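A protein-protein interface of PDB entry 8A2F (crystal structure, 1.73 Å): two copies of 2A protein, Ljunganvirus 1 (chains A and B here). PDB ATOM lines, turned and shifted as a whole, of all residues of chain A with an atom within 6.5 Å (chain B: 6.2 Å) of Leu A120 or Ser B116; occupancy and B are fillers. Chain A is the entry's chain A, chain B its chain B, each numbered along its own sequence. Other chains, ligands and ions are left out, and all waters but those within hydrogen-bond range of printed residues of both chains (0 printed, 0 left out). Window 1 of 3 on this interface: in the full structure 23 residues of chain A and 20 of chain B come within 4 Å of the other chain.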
ATOM      1  N   LYS A  69      -4.935  18.290  18.836  1.00  0.00           N
ATOM      2  CA  LYS A  69      -4.269  17.032  19.154  1.00  0.00           C
ATOM      3  C   LYS A  69      -3.294  17.191  20.332  1.00  0.00           C
ATOM      4  O   LYS A  69      -3.230  16.304  21.174  1.00  0.00           O
ATOM      5  CB  LYS A  69      -3.578  16.513  17.888  1.00  0.00           C
ATOM      6  CG  LYS A  69      -3.003  15.111  17.978  1.00  0.00           C
ATOM      7  CD  LYS A  69      -2.390  14.653  16.688  1.00  0.00           C
ATOM      8  CE  LYS A  69      -1.995  13.197  16.727  1.00  0.00           C
ATOM      9  NZ  LYS A  69      -3.189  12.328  16.643  1.00  0.00           N
ATOM     10  N   TYR A  70      -2.550  18.302  20.399  1.00  0.00           N
ATOM     11  CA  TYR A  70      -1.406  18.422  21.302  1.00  0.00           C
ATOM     12  C   TYR A  70      -1.500  19.542  22.340  1.00  0.00           C
ATOM     13  O   TYR A  70      -0.766  19.511  23.323  1.00  0.00           O
ATOM     14  CB  TYR A  70      -0.136  18.699  20.520  1.00  0.00           C
ATOM     15  CG  TYR A  70       0.260  17.636  19.547  1.00  0.00           C
ATOM     16  CD1 TYR A  70       0.458  16.327  19.961  1.00  0.00           C
ATOM     17  CD2 TYR A  70       0.506  17.943  18.225  1.00  0.00           C
ATOM     18  CE1 TYR A  70       0.886  15.357  19.078  1.00  0.00           C
ATOM     19  CE2 TYR A  70       0.893  16.974  17.316  1.00  0.00           C
ATOM     20  CZ  TYR A  70       1.117  15.681  17.756  1.00  0.00           C
ATOM     21  OH  TYR A  70       1.499  14.728  16.869  1.00  0.00           O
ATOM     22  N   LEU A 115       7.601  19.454  20.210  1.00  0.00           N
ATOM     23  CA  LEU A 115       8.074  18.599  21.304  1.00  0.00           C
ATOM     24  C   LEU A 115       7.178  17.370  21.454  1.00  0.00           C
ATOM     25  O   LEU A 115       7.682  16.249  21.626  1.00  0.00           O
ATOM     26  CB  LEU A 115       8.050  19.396  22.608  1.00  0.00           C
ATOM     27  CG  LEU A 115       9.264  20.232  22.962  1.00  0.00           C
ATOM     28  CD1 LEU A 115       9.132  20.675  24.416  1.00  0.00           C
ATOM     29  CD2 LEU A 115      10.571  19.450  22.794  1.00  0.00           C
ATOM     30  N   SER A 116       5.851  17.578  21.360  1.00  0.00           N
ATOM     31  CA  SER A 116       4.882  16.511  21.578  1.00  0.00           C
ATOM     32  C   SER A 116       4.992  15.469  20.458  1.00  0.00           C
ATOM     33  O   SER A 116       5.021  14.268  20.725  1.00  0.00           O
ATOM     34  CB  SER A 116       3.459  17.049  21.658  1.00  0.00           C
ATOM     35  OG  SER A 116       3.308  17.927  22.767  1.00  0.00           O
ATOM     36  N   ALA A 117       5.012  15.917  19.203  1.00  0.00           N
ATOM     37  CA  ALA A 117       5.126  15.020  18.059  1.00  0.00           C
ATOM     38  C   ALA A 117       6.433  14.217  18.159  1.00  0.00           C
ATOM     39  O   ALA A 117       6.434  12.989  17.947  1.00  0.00           O
ATOM     40  CB  ALA A 117       5.060  15.804  16.773  1.00  0.00           C
ATOM     41  N   SER A 118       7.528  14.900  18.507  1.00  0.00           N
ATOM     42  CA  SER A 118       8.828  14.236  18.629  1.00  0.00           C
ATOM     43  C   SER A 118       8.823  13.177  19.727  1.00  0.00           C
ATOM     44  O   SER A 118       9.293  12.052  19.491  1.00  0.00           O
ATOM     45  CB  SER A 118       9.950  15.195  18.817  1.00  0.00           C
ATOM     46  OG  SER A 118      10.077  16.074  17.722  1.00  0.00           O
ATOM     47  N   LEU A 119       8.264  13.508  20.897  1.00  0.00           N
ATOM     48  CA  LEU A 119       8.187  12.546  21.988  1.00  0.00           C
ATOM     49  C   LEU A 119       7.350  11.334  21.608  1.00  0.00           C
ATOM     50  O   LEU A 119       7.748  10.196  21.861  1.00  0.00           O
ATOM     51  CB  LEU A 119       7.586  13.203  23.230  1.00  0.00           C
ATOM     52  CG  LEU A 119       8.541  14.082  23.999  1.00  0.00           C
ATOM     53  CD1 LEU A 119       7.776  14.926  25.005  1.00  0.00           C
ATOM     54  CD2 LEU A 119       9.593  13.226  24.691  1.00  0.00           C
ATOM     55  N   LEU A 120       6.192  11.566  21.000  1.00  0.00           N
ATOM     56  CA  LEU A 120       5.315  10.440  20.715  1.00  0.00           C
ATOM     57  C   LEU A 120       5.878   9.560  19.600  1.00  0.00           C
ATOM     58  O   LEU A 120       5.536   8.366  19.540  1.00  0.00           O
ATOM     59  CB  LEU A 120       3.924  10.961  20.362  1.00  0.00           C
ATOM     60  CG  LEU A 120       3.208  11.630  21.534  1.00  0.00           C
ATOM     61  CD1 LEU A 120       1.816  12.076  21.100  1.00  0.00           C
ATOM     62  CD2 LEU A 120       3.139  10.732  22.766  1.00  0.00           C
ATOM     63  N   SER A 121       6.779  10.101  18.776  1.00  0.00           N
ATOM     64  CA  SER A 121       7.396   9.285  17.724  1.00  0.00           C
ATOM     65  C   SER A 121       8.321   8.209  18.307  1.00  0.00           C
ATOM     66  O   SER A 121       8.671   7.265  17.605  1.00  0.00           O
ATOM     67  CB  SER A 121       8.139  10.149  16.719  1.00  0.00           C
ATOM     68  OG  SER A 121       9.339  10.672  17.275  1.00  0.00           O
ATOM     69  N   LEU A 122       8.727   8.337  19.579  1.00  0.00           N
ATOM     70  CA  LEU A 122       9.452   7.269  20.253  1.00  0.00           C
ATOM     71  C   LEU A 122       8.665   5.955  20.220  1.00  0.00           C
ATOM     72  O   LEU A 122       9.284   4.887  20.317  1.00  0.00           O
ATOM     73  CB  LEU A 122       9.739   7.669  21.710  1.00  0.00           C
ATOM     74  CG  LEU A 122      10.785   8.771  21.882  1.00  0.00           C
ATOM     75  CD1 LEU A 122      10.721   9.367  23.297  1.00  0.00           C
ATOM     76  CD2 LEU A 122      12.158   8.226  21.601  1.00  0.00           C
ATOM     77  N   LEU A 123       7.338   6.016  20.144  1.00  0.00           N
ATOM     78  CA  LEU A 123       6.503   4.820  20.182  1.00  0.00           C
ATOM     79  C   LEU A 123       6.130   4.314  18.786  1.00  0.00           C
ATOM     80  O   LEU A 123       5.502   3.248  18.675  1.00  0.00           O
ATOM     81  CB  LEU A 123       5.219   5.134  20.948  1.00  0.00           C
ATOM     82  CG  LEU A 123       5.407   5.717  22.348  1.00  0.00           C
ATOM     83  CD1 LEU A 123       4.056   6.117  22.944  1.00  0.00           C
ATOM     84  CD2 LEU A 123       6.128   4.733  23.228  1.00  0.00           C
ATOM     85  N   ALA A 124       6.433   5.106  17.753  1.00  0.00           N
ATOM     86  CA  ALA A 124       5.989   4.803  16.392  1.00  0.00           C
ATOM     87  C   ALA A 124       7.012   3.933  15.678  1.00  0.00           C
ATOM     88  O   ALA A 124       8.219   4.006  15.923  1.00  0.00           O
ATOM     89  CB  ALA A 124       5.781   6.059  15.612  1.00  0.00           C
ATOM     90  N   SER A 131       2.650   9.497  10.855  1.00  0.00           N
ATOM     91  CA  SER A 131       2.361   8.941  12.169  1.00  0.00           C
ATOM     92  C   SER A 131       1.938  10.043  13.144  1.00  0.00           C
ATOM     93  O   SER A 131       2.399  10.068  14.280  1.00  0.00           O
ATOM     94  CB  SER A 131       3.546   8.145  12.697  1.00  0.00           C
ATOM     95  OG  SER A 131       4.750   8.913  12.706  1.00  0.00           O
ATOM     96  N   LYS B  69      -6.805  10.732  20.120  1.00  0.00           N
ATOM     97  CA  LYS B  69      -5.704  11.605  20.489  1.00  0.00           C
ATOM     98  C   LYS B  69      -4.358  10.907  20.291  1.00  0.00           C
ATOM     99  O   LYS B  69      -3.425  11.524  19.798  1.00  0.00           O
ATOM    100  CB  LYS B  69      -5.896  12.068  21.931  1.00  0.00           C
ATOM    101  CG  LYS B  69      -5.028  13.237  22.368  1.00  0.00           C
ATOM    102  CD  LYS B  69      -5.695  14.030  23.478  1.00  0.00           C
ATOM    103  CE  LYS B  69      -4.734  14.849  24.311  1.00  0.00           C
ATOM    104  NZ  LYS B  69      -4.177  16.009  23.573  1.00  0.00           N
ATOM    105  N   TYR B  70      -4.261   9.621  20.650  1.00  0.00           N
ATOM    106  CA  TYR B  70      -2.963   8.952  20.778  1.00  0.00           C
ATOM    107  C   TYR B  70      -2.733   7.780  19.825  1.00  0.00           C
ATOM    108  O   TYR B  70      -1.589   7.329  19.702  1.00  0.00           O
ATOM    109  CB  TYR B  70      -2.801   8.405  22.196  1.00  0.00           C
ATOM    110  CG  TYR B  70      -2.771   9.461  23.268  1.00  0.00           C
ATOM    111  CD1 TYR B  70      -1.891  10.533  23.214  1.00  0.00           C
ATOM    112  CD2 TYR B  70      -3.605   9.356  24.369  1.00  0.00           C
ATOM    113  CE1 TYR B  70      -1.891  11.508  24.199  1.00  0.00           C
ATOM    114  CE2 TYR B  70      -3.606  10.313  25.368  1.00  0.00           C
ATOM    115  CZ  TYR B  70      -2.728  11.381  25.293  1.00  0.00           C
ATOM    116  OH  TYR B  70      -2.741  12.313  26.302  1.00  0.00           O
ATOM    117  N   ASN B  72      -2.999   7.403  16.472  1.00  0.00           N
ATOM    118  CA  ASN B  72      -3.268   8.252  15.319  1.00  0.00           C
ATOM    119  C   ASN B  72      -2.737   7.578  14.062  1.00  0.00           C
ATOM    120  O   ASN B  72      -2.310   8.245  13.116  1.00  0.00           O
ATOM    121  CB  ASN B  72      -2.689   9.651  15.531  1.00  0.00           C
ATOM    122  CG  ASN B  72      -1.269   9.641  16.053  1.00  0.00           C
ATOM    123  OD1 ASN B  72      -0.337   9.280  15.336  1.00  0.00           O
ATOM    124  ND2 ASN B  72      -1.093  10.029  17.305  1.00  0.00           N
ATOM    125  N   GLY B 111      -1.822   0.225  26.111  1.00  0.00           N
ATOM    126  CA  GLY B 111      -0.401   0.444  26.354  1.00  0.00           C
ATOM    127  C   GLY B 111       0.105   1.740  25.722  1.00  0.00           C
ATOM    128  O   GLY B 111       0.867   2.488  26.338  1.00  0.00           O
ATOM    129  N   VAL B 112      -0.299   2.010  24.473  1.00  0.00           N
ATOM    130  CA  VAL B 112       0.176   3.215  23.811  1.00  0.00           C
ATOM    131  C   VAL B 112      -0.441   4.446  24.465  1.00  0.00           C
ATOM    132  O   VAL B 112       0.232   5.471  24.596  1.00  0.00           O
ATOM    133  CB  VAL B 112      -0.080   3.176  22.291  1.00  0.00           C
ATOM    134  CG1 VAL B 112       0.143   4.532  21.636  1.00  0.00           C
ATOM    135  CG2 VAL B 112       0.784   2.111  21.640  1.00  0.00           C
ATOM    136  N   ILE B 113      -1.693   4.357  24.909  1.00  0.00           N
ATOM    137  CA  ILE B 113      -2.286   5.468  25.642  1.00  0.00           C
ATOM    138  C   ILE B 113      -1.451   5.770  26.892  1.00  0.00           C
ATOM    139  O   ILE B 113      -1.117   6.934  27.127  1.00  0.00           O
ATOM    140  CB  ILE B 113      -3.776   5.225  25.960  1.00  0.00           C
ATOM    141  CG1 ILE B 113      -4.629   5.272  24.683  1.00  0.00           C
ATOM    142  CG2 ILE B 113      -4.267   6.226  26.998  1.00  0.00           C
ATOM    143  CD1 ILE B 113      -5.976   4.652  24.799  1.00  0.00           C
ATOM    144  N   LEU B 114      -1.152   4.751  27.702  1.00  0.00           N
ATOM    145  CA  LEU B 114      -0.423   4.964  28.950  1.00  0.00           C
ATOM    146  C   LEU B 114       0.995   5.478  28.695  1.00  0.00           C
ATOM    147  O   LEU B 114       1.456   6.374  29.395  1.00  0.00           O
ATOM    148  CB  LEU B 114      -0.374   3.671  29.767  1.00  0.00           C
ATOM    149  CG  LEU B 114      -1.734   3.106  30.192  1.00  0.00           C
ATOM    150  CD1 LEU B 114      -1.559   1.811  30.983  1.00  0.00           C
ATOM    151  CD2 LEU B 114      -2.505   4.124  31.013  1.00  0.00           C
ATOM    152  N   LEU B 115       1.713   4.892  27.724  1.00  0.00           N
ATOM    153  CA  LEU B 115       3.057   5.361  27.417  1.00  0.00           C
ATOM    154  C   LEU B 115       3.032   6.797  26.887  1.00  0.00           C
ATOM    155  O   LEU B 115       3.918   7.586  27.215  1.00  0.00           O
ATOM    156  CB  LEU B 115       3.715   4.436  26.397  1.00  0.00           C
ATOM    157  CG  LEU B 115       4.192   3.096  26.960  1.00  0.00           C
ATOM    158  CD1 LEU B 115       4.699   2.186  25.850  1.00  0.00           C
ATOM    159  CD2 LEU B 115       5.266   3.296  28.030  1.00  0.00           C
ATOM    160  N   SER B 116       2.028   7.131  26.057  1.00  0.00           N
ATOM    161  CA  SER B 116       1.888   8.473  25.498  1.00  0.00           C
ATOM    162  C   SER B 116       1.667   9.505  26.609  1.00  0.00           C
ATOM    163  O   SER B 116       2.334  10.539  26.639  1.00  0.00           O
ATOM    164  CB  SER B 116       0.782   8.529  24.460  1.00  0.00           C
ATOM    165  OG  SER B 116       1.066   7.677  23.347  1.00  0.00           O
ATOM    166  N   ALA B 117       0.730   9.214  27.519  1.00  0.00           N
ATOM    167  CA  ALA B 117       0.466  10.108  28.641  1.00  0.00           C
ATOM    168  C   ALA B 117       1.730  10.310  29.486  1.00  0.00           C
ATOM    169  O   ALA B 117       2.073  11.438  29.870  1.00  0.00           O
ATOM    170  CB  ALA B 117      -0.673   9.548  29.462  1.00  0.00           C
ATOM    171  N   SER B 118       2.434   9.211  29.775  1.00  0.00           N
ATOM    172  CA  SER B 118       3.651   9.279  30.579  1.00  0.00           C
ATOM    173  C   SER B 118       4.741  10.107  29.904  1.00  0.00           C
ATOM    174  O   SER B 118       5.389  10.920  30.555  1.00  0.00           O
ATOM    175  CB  SER B 118       4.166   7.901  30.931  1.00  0.00           C
ATOM    176  OG  SER B 118       3.183   7.174  31.665  1.00  0.00           O
ATOM    177  N   LEU B 119       4.952   9.919  28.601  1.00  0.00           N
ATOM    178  CA  LEU B 119       5.949  10.695  27.874  1.00  0.00           C
ATOM    179  C   LEU B 119       5.606  12.184  27.871  1.00  0.00           C
ATOM    180  O   LEU B 119       6.477  13.030  28.086  1.00  0.00           O
ATOM    181  CB  LEU B 119       6.086  10.187  26.437  1.00  0.00           C
ATOM    182  CG  LEU B 119       6.898   8.908  26.279  1.00  0.00           C
ATOM    183  CD1 LEU B 119       6.745   8.357  24.860  1.00  0.00           C
ATOM    184  CD2 LEU B 119       8.344   9.154  26.594  1.00  0.00           C
ATOM    185  N   LEU B 120       4.342  12.518  27.625  1.00  0.00           N
ATOM    186  CA  LEU B 120       3.983  13.925  27.574  1.00  0.00           C
ATOM    187  C   LEU B 120       4.055  14.571  28.954  1.00  0.00           C
ATOM    188  O   LEU B 120       4.202  15.788  29.049  1.00  0.00           O
ATOM    189  CB  LEU B 120       2.586  14.065  26.968  1.00  0.00           C
ATOM    190  CG  LEU B 120       2.482  13.666  25.503  1.00  0.00           C
ATOM    191  CD1 LEU B 120       1.049  13.802  25.010  1.00  0.00           C
ATOM    192  CD2 LEU B 120       3.425  14.486  24.635  1.00  0.00           C
ATOM    193  N   SER B 121       3.963  13.792  30.033  1.00  0.00           N
ATOM    194  CA  SER B 121       4.062  14.349  31.379  1.00  0.00           C
ATOM    195  C   SER B 121       5.453  14.920  31.664  1.00  0.00           C
ATOM    196  O   SER B 121       5.622  15.697  32.616  1.00  0.00           O
ATOM    197  CB  SER B 121       3.676  13.318  32.424  1.00  0.00           C
ATOM    198  OG  SER B 121       4.734  12.357  32.645  1.00  0.00           O
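Among the printed residues, pairs that only touch across the chains: Ser A116 with Leu B120 (3.9 Å), Leu A119 with Leu B119 (3.7 Å), Leu A120 with Ser B116 (3.6 Å), Leu A123 with Leu B115 (3.9 Å), Leu A123 with Ser B116 (3.4 Å) and Leu A123 with Leu B119 (3.9 Å).
Ser B116 touches just these residues of chain A: Leu A120 (3.6 Å) and Leu A123 (3.4 Å).
Printed residues of chain A within 4 Å of Asn B72: Lys A69 and Ser A131.
Of the printed residues of chain B, Ser A131 touches Asn B72.
Printed residues of chain B within 4 Å of Lys A69: Lys B69 (2.6 Å) and Asn B72 (2.9 Å).
Of the printed residues of chain A, Leu B120 touches Ser A116.
Of the printed residues of chain A, Leu B115 touches Leu A123 (3.9 Å).
The nearest residue of chain B that does not touch Leu A120 is Leu B120 (4.1 Å).
The nearest printed residue of chain A that does not touch Ser B116 is Leu A119 (6.8 Å).
Of the 13 printed residues of chain A, 6 touch a printed residue of chain B.
Printed residues of chain A that touch a printed residue of chain B: Lys A69, Ser A116, Leu A119, Leu A120, Leu A123 and Ser A131.
Hydrophobic or aromatic side chains of chain A that line the printed part of chain B: Leu A119, Leu A120 and Leu A123.
Of the 14 printed residues of chain B, 6 touch a printed residue of chain A.
Among the printed residues, no Asp or Glu carboxylate lies within 4 Å of a Lys or Arg side-chain nitrogen of the other chain.
Lys B69 touches its own counterpart, Lys A69.
Ser A116 touches Leu B120, and with the chains exchanged Leu A120 touches Ser B116.
Leu A119 touches its own counterpart, Leu B119.
Positions printed for both chains: 69, 70, 115, 116, 117, 118, 119, 120 and 121.
Of the 9 pairs that touch across the chains among the printed residues, 4 have their exchanged pair printed and touching as well.
O of Val B112 lies within hydrogen-bond range of OG of Ser B116 (2.7 Å).
The backbone carbonyl oxygen of Lys A69 is in hydrogen-bond range of the side-chain amino group of Lys B69, at 2.6 Å.
OD1 of Asn B72 sits close to O of Ser A131 (3.0 Å).
ND2 of Asn B72 lies close to NZ of Lys A69.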
